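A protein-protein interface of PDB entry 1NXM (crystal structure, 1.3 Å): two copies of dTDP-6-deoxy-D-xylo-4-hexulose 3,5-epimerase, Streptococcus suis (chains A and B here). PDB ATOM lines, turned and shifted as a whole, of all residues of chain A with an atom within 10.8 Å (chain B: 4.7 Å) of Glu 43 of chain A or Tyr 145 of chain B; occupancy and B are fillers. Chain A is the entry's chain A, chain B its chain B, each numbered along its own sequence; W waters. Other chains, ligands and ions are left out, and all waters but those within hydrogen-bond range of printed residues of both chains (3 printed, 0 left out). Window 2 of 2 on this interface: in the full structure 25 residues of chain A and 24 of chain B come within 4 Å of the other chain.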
ATOM      1  N   LEU A  10      10.570  13.133  -4.861  1.00  0.00           N
ATOM      2  CA  LEU A  10       9.529  13.801  -5.619  1.00  0.00           C
ATOM      3  C   LEU A  10       9.520  15.300  -5.279  1.00  0.00           C
ATOM      4  O   LEU A  10       9.424  15.669  -4.116  1.00  0.00           O
ATOM      5  CB  LEU A  10       8.171  13.171  -5.303  1.00  0.00           C
ATOM      6  CG  LEU A  10       6.980  13.824  -6.014  1.00  0.00           C
ATOM      7  CD1 LEU A  10       7.022  13.555  -7.513  1.00  0.00           C
ATOM      8  CD2 LEU A  10       5.646  13.341  -5.424  1.00  0.00           C
ATOM      9  N   PHE A  24       9.322  18.444 -12.714  1.00  0.00           N
ATOM     10  CA  PHE A  24       9.267  17.507 -11.614  1.00  0.00           C
ATOM     11  C   PHE A  24      10.400  16.508 -11.649  1.00  0.00           C
ATOM     12  O   PHE A  24      10.706  15.921 -12.681  1.00  0.00           O
ATOM     13  CB  PHE A  24       7.971  16.708 -11.603  1.00  0.00           C
ATOM     14  CG  PHE A  24       6.739  17.529 -11.405  1.00  0.00           C
ATOM     15  CD1 PHE A  24       6.154  18.178 -12.462  1.00  0.00           C
ATOM     16  CD2 PHE A  24       6.195  17.693 -10.143  1.00  0.00           C
ATOM     17  CE1 PHE A  24       5.029  18.932 -12.296  1.00  0.00           C
ATOM     18  CE2 PHE A  24       5.035  18.488  -9.986  1.00  0.00           C
ATOM     19  CZ  PHE A  24       4.489  19.106 -11.074  1.00  0.00           C
ATOM     20  N   GLU A  38       6.151   5.928  -9.845  1.00  0.00           N
ATOM     21  CA  GLU A  38       4.853   6.586  -9.882  1.00  0.00           C
ATOM     22  C   GLU A  38       5.034   7.837 -10.733  1.00  0.00           C
ATOM     23  O   GLU A  38       5.538   8.861 -10.276  1.00  0.00           O
ATOM     24  CB  GLU A  38       4.366   6.926  -8.480  1.00  0.00           C
ATOM     25  CG  GLU A  38       4.356   5.768  -7.530  1.00  0.00           C
ATOM     26  CD  GLU A  38       3.717   6.082  -6.194  1.00  0.00           C
ATOM     27  OE1 GLU A  38       3.569   7.280  -5.850  1.00  0.00           O
ATOM     28  OE2 GLU A  38       3.402   5.085  -5.514  1.00  0.00           O
ATOM     29  N   ASN A  39       4.720   7.723 -12.011  1.00  0.00           N
ATOM     30  CA  ASN A  39       4.893   8.809 -12.954  1.00  0.00           C
ATOM     31  C   ASN A  39       4.000  10.021 -12.698  1.00  0.00           C
ATOM     32  O   ASN A  39       4.391  11.147 -12.985  1.00  0.00           O
ATOM     33  CB  ASN A  39       4.630   8.293 -14.364  1.00  0.00           C
ATOM     34  CG  ASN A  39       4.964   9.297 -15.403  1.00  0.00           C
ATOM     35  OD1 ASN A  39       6.108   9.779 -15.479  1.00  0.00           O
ATOM     36  ND2 ASN A  39       3.984   9.612 -16.244  1.00  0.00           N
ATOM     37  N   PHE A  40       2.793   9.787 -12.222  1.00  0.00           N
ATOM     38  CA  PHE A  40       1.854  10.831 -11.859  1.00  0.00           C
ATOM     39  C   PHE A  40       1.073  10.356 -10.659  1.00  0.00           C
ATOM     40  O   PHE A  40       0.597   9.231 -10.622  1.00  0.00           O
ATOM     41  CB  PHE A  40       0.916  11.162 -13.027  1.00  0.00           C
ATOM     42  CG  PHE A  40      -0.009  12.272 -12.702  1.00  0.00           C
ATOM     43  CD1 PHE A  40       0.459  13.569 -12.691  1.00  0.00           C
ATOM     44  CD2 PHE A  40      -1.300  12.026 -12.282  1.00  0.00           C
ATOM     45  CE1 PHE A  40      -0.369  14.620 -12.326  1.00  0.00           C
ATOM     46  CE2 PHE A  40      -2.136  13.090 -11.932  1.00  0.00           C
ATOM     47  CZ  PHE A  40      -1.646  14.368 -11.954  1.00  0.00           C
ATOM     48  N   GLN A  41       0.924  11.219  -9.668  1.00  0.00           N
ATOM     49  CA  GLN A  41       0.158  10.894  -8.478  1.00  0.00           C
ATOM     50  C   GLN A  41      -0.555  12.172  -8.038  1.00  0.00           C
ATOM     51  O   GLN A  41       0.066  13.116  -7.586  1.00  0.00           O
ATOM     52  CB  GLN A  41       1.091  10.290  -7.407  1.00  0.00           C
ATOM     53  CG  GLN A  41       0.441   9.282  -6.511  1.00  0.00           C
ATOM     54  CD  GLN A  41      -0.335   9.897  -5.372  1.00  0.00           C
ATOM     55  OE1 GLN A  41      -0.854  11.012  -5.494  1.00  0.00           O
ATOM     56  NE2 GLN A  41      -0.399   9.194  -4.244  1.00  0.00           N
ATOM     57  N   LYS A  42      -1.851  12.265  -8.325  1.00  0.00           N
ATOM     58  CA  LYS A  42      -2.575  13.537  -8.229  1.00  0.00           C
ATOM     59  C   LYS A  42      -2.527  14.114  -6.808  1.00  0.00           C
ATOM     60  O   LYS A  42      -2.311  15.297  -6.612  1.00  0.00           O
ATOM     61  CB  LYS A  42      -4.030  13.341  -8.667  1.00  0.00           C
ATOM     62  CG  LYS A  42      -4.912  14.568  -8.610  1.00  0.00           C
ATOM     63  CD  LYS A  42      -6.305  14.218  -9.081  1.00  0.00           C
ATOM     64  CE  LYS A  42      -7.260  15.363  -8.968  1.00  0.00           C
ATOM     65  NZ  LYS A  42      -8.574  14.966  -9.595  1.00  0.00           N
ATOM     66  N   GLU A  43      -2.734  13.264  -5.817  1.00  0.00           N
ATOM     67  CA  GLU A  43      -2.755  13.694  -4.413  1.00  0.00           C
ATOM     68  C   GLU A  43      -1.421  14.272  -3.927  1.00  0.00           C
ATOM     69  O   GLU A  43      -1.402  15.236  -3.161  1.00  0.00           O
ATOM     70  CB  GLU A  43      -3.200  12.527  -3.519  1.00  0.00           C
ATOM     71  CG  GLU A  43      -3.542  12.855  -2.087  1.00  0.00           C
ATOM     72  CD  GLU A  43      -4.303  11.721  -1.391  1.00  0.00           C
ATOM     73  OE1 GLU A  43      -3.670  10.711  -1.005  1.00  0.00           O
ATOM     74  OE2 GLU A  43      -5.534  11.832  -1.249  1.00  0.00           O
ATOM     75  N   LYS A  44      -0.321  13.718  -4.391  1.00  0.00           N
ATOM     76  CA  LYS A  44       0.971  14.259  -4.036  1.00  0.00           C
ATOM     77  C   LYS A  44       1.370  15.439  -4.910  1.00  0.00           C
ATOM     78  O   LYS A  44       2.049  16.346  -4.428  1.00  0.00           O
ATOM     79  CB  LYS A  44       2.023  13.157  -4.055  1.00  0.00           C
ATOM     80  CG  LYS A  44       1.732  12.076  -3.017  1.00  0.00           C
ATOM     81  CD  LYS A  44       2.827  11.031  -2.926  1.00  0.00           C
ATOM     82  CE  LYS A  44       2.635  10.137  -1.696  1.00  0.00           C
ATOM     83  NZ  LYS A  44       3.026  10.833  -0.425  1.00  0.00           N
ATOM     84  N   MET A  45       0.938  15.476  -6.171  1.00  0.00           N
ATOM     85  CA  MET A  45       1.460  16.520  -7.050  1.00  0.00           C
ATOM     86  C   MET A  45       0.708  17.833  -6.921  1.00  0.00           C
ATOM     87  O   MET A  45       1.280  18.888  -7.177  1.00  0.00           O
ATOM     88  CB  MET A  45       1.605  16.000  -8.471  1.00  0.00           C
ATOM     89  CG  MET A  45       2.686  14.922  -8.517  1.00  0.00           C
ATOM     90  SD  MET A  45       2.821  14.141 -10.090  1.00  0.00           S
ATOM     91  CE  MET A  45       3.246  15.522 -11.127  1.00  0.00           C
ATOM     92  N   LEU A  46      -0.543  17.798  -6.472  1.00  0.00           N
ATOM     93  CA  LEU A  46      -1.269  19.062  -6.242  1.00  0.00           C
ATOM     94  C   LEU A  46      -0.519  19.969  -5.236  1.00  0.00           C
ATOM     95  O   LEU A  46      -0.284  21.160  -5.511  1.00  0.00           O
ATOM     96  CB  LEU A  46      -2.716  18.779  -5.811  1.00  0.00           C
ATOM     97  CG  LEU A  46      -3.667  18.295  -6.901  1.00  0.00           C
ATOM     98  CD1 LEU A  46      -5.014  17.841  -6.343  1.00  0.00           C
ATOM     99  CD2 LEU A  46      -3.880  19.385  -7.908  1.00  0.00           C
ATOM    100  N   PRO A  47      -0.126  19.456  -4.064  1.00  0.00           N
ATOM    101  CA  PRO A  47       0.621  20.328  -3.125  1.00  0.00           C
ATOM    102  C   PRO A  47       1.985  20.824  -3.607  1.00  0.00           C
ATOM    103  O   PRO A  47       2.500  21.796  -3.084  1.00  0.00           O
ATOM    104  CB  PRO A  47       0.780  19.474  -1.853  1.00  0.00           C
ATOM    105  CG  PRO A  47      -0.063  18.300  -2.028  1.00  0.00           C
ATOM    106  CD  PRO A  47      -0.420  18.149  -3.461  1.00  0.00           C
ATOM    107  N   LEU A  48       2.575  20.159  -4.594  1.00  0.00           N
ATOM    108  CA  LEU A  48       3.827  20.620  -5.210  1.00  0.00           C
ATOM    109  C   LEU A  48       3.625  21.701  -6.266  1.00  0.00           C
ATOM    110  O   LEU A  48       4.587  22.213  -6.832  1.00  0.00           O
ATOM    111  CB  LEU A  48       4.558  19.445  -5.848  1.00  0.00           C
ATOM    112  CG  LEU A  48       4.986  18.391  -4.832  1.00  0.00           C
ATOM    113  CD1 LEU A  48       5.609  17.215  -5.537  1.00  0.00           C
ATOM    114  CD2 LEU A  48       5.942  18.935  -3.791  1.00  0.00           C
ATOM    115  N   GLY A  49       2.369  22.005  -6.573  1.00  0.00           N
ATOM    116  CA  GLY A  49       2.027  23.069  -7.484  1.00  0.00           C
ATOM    117  C   GLY A  49       1.387  22.613  -8.786  1.00  0.00           C
ATOM    118  O   GLY A  49       1.047  23.448  -9.599  1.00  0.00           O
ATOM    119  N   PHE A  50       1.220  21.318  -9.015  1.00  0.00           N
ATOM    120  CA  PHE A  50       0.479  20.875 -10.200  1.00  0.00           C
ATOM    121  C   PHE A  50      -0.910  21.530 -10.150  1.00  0.00           C
ATOM    122  O   PHE A  50      -1.592  21.422  -9.111  1.00  0.00           O
ATOM    123  CB  PHE A  50       0.374  19.345 -10.251  1.00  0.00           C
ATOM    124  CG  PHE A  50      -0.097  18.830 -11.568  1.00  0.00           C
ATOM    125  CD1 PHE A  50       0.789  18.340 -12.496  1.00  0.00           C
ATOM    126  CD2 PHE A  50      -1.435  18.829 -11.885  1.00  0.00           C
ATOM    127  CE1 PHE A  50       0.335  17.880 -13.723  1.00  0.00           C
ATOM    128  CE2 PHE A  50      -1.875  18.361 -13.106  1.00  0.00           C
ATOM    129  CZ  PHE A  50      -0.990  17.895 -14.022  1.00  0.00           C
ATOM    130  N   PRO A  51      -1.328  22.263 -11.191  1.00  0.00           N
ATOM    131  CA  PRO A  51      -2.527  23.106 -11.041  1.00  0.00           C
ATOM    132  C   PRO A  51      -3.848  22.347 -10.979  1.00  0.00           C
ATOM    133  O   PRO A  51      -4.098  21.476 -11.815  1.00  0.00           O
ATOM    134  CB  PRO A  51      -2.468  24.028 -12.263  1.00  0.00           C
ATOM    135  CG  PRO A  51      -1.709  23.261 -13.256  1.00  0.00           C
ATOM    136  CD  PRO A  51      -0.686  22.439 -12.508  1.00  0.00           C
ATOM    137  N   GLU A  52      -4.686  22.699 -10.005  1.00  0.00           N
ATOM    138  CA  GLU A  52      -6.045  22.148  -9.941  1.00  0.00           C
ATOM    139  C   GLU A  52      -6.822  22.388 -11.239  1.00  0.00           C
ATOM    140  O   GLU A  52      -7.644  21.565 -11.628  1.00  0.00           O
ATOM    141  CB  GLU A  52      -6.855  22.712  -8.759  1.00  0.00           C
ATOM    142  CG  GLU A  52      -8.244  22.078  -8.584  1.00  0.00           C
ATOM    143  CD  GLU A  52      -8.239  20.554  -8.459  1.00  0.00           C
ATOM    144  OE1 GLU A  52      -7.420  20.011  -7.683  1.00  0.00           O
ATOM    145  OE2 GLU A  52      -9.065  19.881  -9.149  1.00  0.00           O
ATOM    146  N   PHE A  55      -7.667  19.699 -13.906  1.00  0.00           N
ATOM    147  CA  PHE A  55      -8.753  18.769 -13.691  1.00  0.00           C
ATOM    148  C   PHE A  55     -10.138  19.343 -13.739  1.00  0.00           C
ATOM    149  O   PHE A  55     -11.106  18.610 -13.550  1.00  0.00           O
ATOM    150  CB  PHE A  55      -8.564  18.152 -12.311  1.00  0.00           C
ATOM    151  CG  PHE A  55      -7.230  17.507 -12.148  1.00  0.00           C
ATOM    152  CD1 PHE A  55      -6.201  18.156 -11.475  1.00  0.00           C
ATOM    153  CD2 PHE A  55      -7.002  16.269 -12.709  1.00  0.00           C
ATOM    154  CE1 PHE A  55      -4.979  17.561 -11.369  1.00  0.00           C
ATOM    155  CE2 PHE A  55      -5.766  15.679 -12.602  1.00  0.00           C
ATOM    156  CZ  PHE A  55      -4.773  16.330 -11.939  1.00  0.00           C
ATOM    157  N   LEU A  60      -9.593  13.856 -19.814  1.00  0.00           N
ATOM    158  CA  LEU A  60      -8.329  13.161 -19.694  1.00  0.00           C
ATOM    159  C   LEU A  60      -8.033  12.357 -20.941  1.00  0.00           C
ATOM    160  O   LEU A  60      -8.851  11.555 -21.399  1.00  0.00           O
ATOM    161  CB  LEU A  60      -8.364  12.228 -18.499  1.00  0.00           C
ATOM    162  CG  LEU A  60      -7.056  11.526 -18.197  1.00  0.00           C
ATOM    163  CD1 LEU A  60      -6.001  12.503 -17.738  1.00  0.00           C
ATOM    164  CD2 LEU A  60      -7.304  10.446 -17.155  1.00  0.00           C
ATOM    165  N   GLY B  58     -12.529  10.972  -8.315  1.00  0.00           N
ATOM    166  CA  GLY B  58     -11.608  11.982  -8.841  1.00  0.00           C
ATOM    167  C   GLY B  58     -10.139  11.715  -8.563  1.00  0.00           C
ATOM    168  O   GLY B  58      -9.328  12.636  -8.490  1.00  0.00           O
ATOM    169  N   LYS B  59      -9.787  10.450  -8.383  1.00  0.00           N
ATOM    170  CA  LYS B  59      -8.418  10.079  -8.049  1.00  0.00           C
ATOM    171  C   LYS B  59      -7.711   9.547  -9.280  1.00  0.00           C
ATOM    172  O   LYS B  59      -8.312   8.846 -10.101  1.00  0.00           O
ATOM    173  CB  LYS B  59      -8.432   9.011  -6.974  1.00  0.00           C
ATOM    174  CG  LYS B  59      -9.017   9.496  -5.652  1.00  0.00           C
ATOM    175  CD  LYS B  59      -9.098   8.353  -4.670  1.00  0.00           C
ATOM    176  CE  LYS B  59      -9.757   8.750  -3.373  1.00  0.00           C
ATOM    177  NZ  LYS B  59     -10.075   7.542  -2.543  1.00  0.00           N
ATOM    178  N   LEU B  60      -6.420   9.851  -9.409  1.00  0.00           N
ATOM    179  CA  LEU B  60      -5.666   9.418 -10.565  1.00  0.00           C
ATOM    180  C   LEU B  60      -4.195   9.248 -10.232  1.00  0.00           C
ATOM    181  O   LEU B  60      -3.570  10.123  -9.656  1.00  0.00           O
ATOM    182  CB  LEU B  60      -5.826  10.437 -11.711  1.00  0.00           C
ATOM    183  CG  LEU B  60      -5.179  10.064 -13.048  1.00  0.00           C
ATOM    184  CD1 LEU B  60      -5.860   8.875 -13.663  1.00  0.00           C
ATOM    185  CD2 LEU B  60      -5.202  11.244 -13.999  1.00  0.00           C
ATOM    186  N   GLN B  61      -3.652   8.130 -10.675  1.00  0.00           N
ATOM    187  CA  GLN B  61      -2.230   7.829 -10.564  1.00  0.00           C
ATOM    188  C   GLN B  61      -1.814   7.000 -11.766  1.00  0.00           C
ATOM    189  O   GLN B  61      -2.560   6.150 -12.213  1.00  0.00           O
ATOM    190  CB  GLN B  61      -1.953   7.099  -9.234  1.00  0.00           C
ATOM    191  CG  GLN B  61      -0.517   6.618  -9.042  1.00  0.00           C
ATOM    192  CD  GLN B  61      -0.285   5.959  -7.698  1.00  0.00           C
ATOM    193  OE1 GLN B  61      -1.073   6.227  -6.769  1.00  0.00           O
ATOM    194  NE2 GLN B  61       0.704   5.185  -7.553  1.00  0.00           N
ATOM    195  N   TRP B  80      -7.692  -0.927  -5.915  1.00  0.00           N
ATOM    196  CA  TRP B  80      -8.061   0.048  -6.909  1.00  0.00           C
ATOM    197  C   TRP B  80      -8.228  -0.643  -8.228  1.00  0.00           C
ATOM    198  O   TRP B  80      -7.685  -1.722  -8.453  1.00  0.00           O
ATOM    199  CB  TRP B  80      -7.021   1.148  -6.989  1.00  0.00           C
ATOM    200  CG  TRP B  80      -5.599   0.689  -6.849  1.00  0.00           C
ATOM    201  CD1 TRP B  80      -4.860   0.034  -7.772  1.00  0.00           C
ATOM    202  CD2 TRP B  80      -4.781   0.808  -5.679  1.00  0.00           C
ATOM    203  NE1 TRP B  80      -3.616  -0.253  -7.263  1.00  0.00           N
ATOM    204  CE2 TRP B  80      -3.543   0.225  -5.976  1.00  0.00           C
ATOM    205  CE3 TRP B  80      -4.967   1.388  -4.415  1.00  0.00           C
ATOM    206  CZ2 TRP B  80      -2.493   0.187  -5.059  1.00  0.00           C
ATOM    207  CZ3 TRP B  80      -3.928   1.330  -3.485  1.00  0.00           C
ATOM    208  CH2 TRP B  80      -2.706   0.754  -3.823  1.00  0.00           C
ATOM    209  N   ASP B 144      -7.074   4.966  -7.057  1.00  0.00           N
ATOM    210  CA  ASP B 144      -6.963   5.204  -5.624  1.00  0.00           C
ATOM    211  C   ASP B 144      -5.486   5.174  -5.249  1.00  0.00           C
ATOM    212  O   ASP B 144      -4.665   4.772  -6.051  1.00  0.00           O
ATOM    213  CB  ASP B 144      -7.782   4.168  -4.841  1.00  0.00           C
ATOM    214  CG  ASP B 144      -8.368   4.712  -3.539  1.00  0.00           C
ATOM    215  OD1 ASP B 144      -7.930   5.774  -3.038  1.00  0.00           O
ATOM    216  OD2 ASP B 144      -9.280   4.089  -2.952  1.00  0.00           O
ATOM    217  N   TYR B 145      -5.182   5.608  -4.032  1.00  0.00           N
ATOM    218  CA  TYR B 145      -3.829   5.738  -3.524  1.00  0.00           C
ATOM    219  C   TYR B 145      -3.656   4.862  -2.310  1.00  0.00           C
ATOM    220  O   TYR B 145      -4.610   4.580  -1.579  1.00  0.00           O
ATOM    221  CB  TYR B 145      -3.567   7.190  -3.096  1.00  0.00           C
ATOM    222  CG  TYR B 145      -4.107   8.225  -4.072  1.00  0.00           C
ATOM    223  CD1 TYR B 145      -5.099   9.117  -3.685  1.00  0.00           C
ATOM    224  CD2 TYR B 145      -3.631   8.311  -5.387  1.00  0.00           C
ATOM    225  CE1 TYR B 145      -5.598  10.060  -4.561  1.00  0.00           C
ATOM    226  CE2 TYR B 145      -4.130   9.254  -6.244  1.00  0.00           C
ATOM    227  CZ  TYR B 145      -5.103  10.123  -5.847  1.00  0.00           C
ATOM    228  OH  TYR B 145      -5.586  11.065  -6.736  1.00  0.00           O
ATOM    229  N   TRP B 146      -2.427   4.472  -2.041  1.00  0.00           N
ATOM    230  CA  TRP B 146      -2.146   3.731  -0.830  1.00  0.00           C
ATOM    231  C   TRP B 146      -2.648   4.450   0.411  1.00  0.00           C
ATOM    232  O   TRP B 146      -2.464   5.649   0.579  1.00  0.00           O
ATOM    233  CB  TRP B 146      -0.636   3.484  -0.662  1.00  0.00           C
ATOM    234  CG  TRP B 146      -0.320   2.680   0.598  1.00  0.00           C
ATOM    235  CD1 TRP B 146      -0.236   1.325   0.690  1.00  0.00           C
ATOM    236  CD2 TRP B 146      -0.102   3.182   1.935  1.00  0.00           C
ATOM    237  NE1 TRP B 146       0.045   0.953   1.980  1.00  0.00           N
ATOM    238  CE2 TRP B 146       0.111   2.069   2.772  1.00  0.00           C
ATOM    239  CE3 TRP B 146      -0.072   4.461   2.508  1.00  0.00           C
ATOM    240  CZ2 TRP B 146       0.385   2.194   4.133  1.00  0.00           C
ATOM    241  CZ3 TRP B 146       0.187   4.586   3.865  1.00  0.00           C
ATOM    242  CH2 TRP B 146       0.399   3.457   4.667  1.00  0.00           C
ATOM    243  N   ALA B 147      -3.269   3.687   1.296  1.00  0.00           N
ATOM    244  CA  ALA B 147      -3.615   4.160   2.612  1.00  0.00           C
ATOM    245  C   ALA B 147      -3.643   2.941   3.478  1.00  0.00           C
ATOM    246  O   ALA B 147      -4.009   1.849   3.027  1.00  0.00           O
ATOM    247  CB  ALA B 147      -4.963   4.834   2.610  1.00  0.00           C
ATOM    248  N   LEU B 150      -6.678   0.655   3.601  1.00  0.00           N
ATOM    249  CA  LEU B 150      -6.973  -0.219   2.485  1.00  0.00           C
ATOM    250  C   LEU B 150      -6.274  -1.584   2.573  1.00  0.00           C
ATOM    251  O   LEU B 150      -6.530  -2.441   1.755  1.00  0.00           O
ATOM    252  CB  LEU B 150      -6.587   0.479   1.177  1.00  0.00           C
ATOM    253  CG  LEU B 150      -7.629   1.255   0.379  1.00  0.00           C
ATOM    254  CD1 LEU B 150      -8.770   1.901   1.117  1.00  0.00           C
ATOM    255  CD2 LEU B 150      -6.905   2.298  -0.461  1.00  0.00           C
HETATM  256  O   HOH W   1       2.880   2.833  -6.320  1.00  0.00           O
HETATM  257  O   HOH W   2      -4.339   8.502   0.485  1.00  0.00           O
HETATM  258  O   HOH W   3     -10.070  15.240  -7.030  1.00  0.00           O
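OE2 of Glu 38 of chain A lies within hydrogen-bond range of NE2 of Gln 61 of chain B, at 3.4 Å.
NZ of Lys 42 of chain A is in hydrogen-bond range of O of Gly 58 of chain B (2.7 Å).
O of Leu 60 of chain B is in hydrogen-bond range of N of Lys 42 of chain A, 3.1 Å away.
The backbone NH of Glu 43 of chain A sits at hydrogen-bond distance from the side-chain amide oxygen of Gln 41 of chain A (3.0 Å).
The side-chain amide oxygen (OE1) of Gln 41 of chain A lies within hydrogen-bond range of the backbone NH (N) of Lys 44 of chain A.
The side-chain sulfur (SD) of Met 45 of chain A lies within hydrogen-bond range of the backbone NH (N) of Gln 41 of chain A.
N of Leu 60 of chain B lies within hydrogen-bond range of OH of Tyr 145 of chain B (3.1 Å).
O of Leu 60 of chain B touches CD2 of Phe 40 of chain A, at 3.96 Å.
Gln 61 of chain B touches Phe 40 of chain A.
Leu 60 of chain B touches Gln 41 of chain A.
Gln 61 of chain B touches Gln 41 of chain A.
CD2 of Tyr 145 of chain B touches NE2 of Gln 41 of chain A (3.5 Å).
Lys 42 of chain A touches Tyr 145 of chain B (CB to OH, 3.4 Å).
Glu 43 of chain A touches Tyr 145 of chain B.
Leu 60 of chain A touches Leu 60 of chain B (CD2 to CD2, 3.9 Å).
Glu 43 of chain A touches just one residue of chain B: Tyr 145.
Tyr 145 of chain B touches just these residues of chain A: Gln 41 (3.5 Å), Lys 42 (3.4 Å) and Glu 43 (3.4 Å).
No residue of chain A comes within 4 Å of Lys 59 of chain B.
No residue of chain A comes within 4 Å of Asp 144 of chain B.
Of the printed residues of chain B, Gln 41 of chain A touches Leu 60, Gln 61 and Tyr 145.
Of the printed residues of chain B, Lys 42 of chain A touches Gly 58 (2.7 Å), Leu 60 (3.1 Å) and Tyr 145 (3.4 Å).
Of the printed residues of chain A, Gln 61 of chain B touches Glu 38, Phe 40 and Gln 41.
Phe 24 of chain A touches none of the printed residues of chain B.
Glu 52 of chain A touches none of the printed residues of chain B.
The nearest printed residue of chain B that does not touch Glu 43 of chain A is Leu 60 of chain B (5.0 Å).
The nearest printed residue of chain A that does not touch Tyr 145 of chain B is Lys 44 of chain A (6.2 Å).
Printed residues of chain A that touch a printed residue of chain B: Glu 38, Phe 40, Gln 41, Lys 42, Glu 43 and Leu 60.
Hydrophobic or aromatic side chains of chain A that line the printed part of chain B: Phe 40 and Leu 60.
Hydrophobic or aromatic side chains of chain B that line the printed part of chain A: Leu 60 and Tyr 145.
Leu 60 of chain B touches its own counterpart, Leu 60 of chain A.
Position printed for both chains: 60.
Water W1 bridges the side-chain carboxylate of Glu 38 of chain A (2.4 Å) and the side-chain amide nitrogen of Gln 61 of chain B (3.4 Å).
Water W2 lies within hydrogen-bond range of OE1 of Glu 43 of chain A (2.7 Å) and O of Trp 146 of chain B (3.4 Å).
Water W3 bridges the side-chain amino group of Lys 42 of chain A (3.0 Å) and the backbone carbonyl oxygen of Gly 58 of chain B (3.1 Å).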
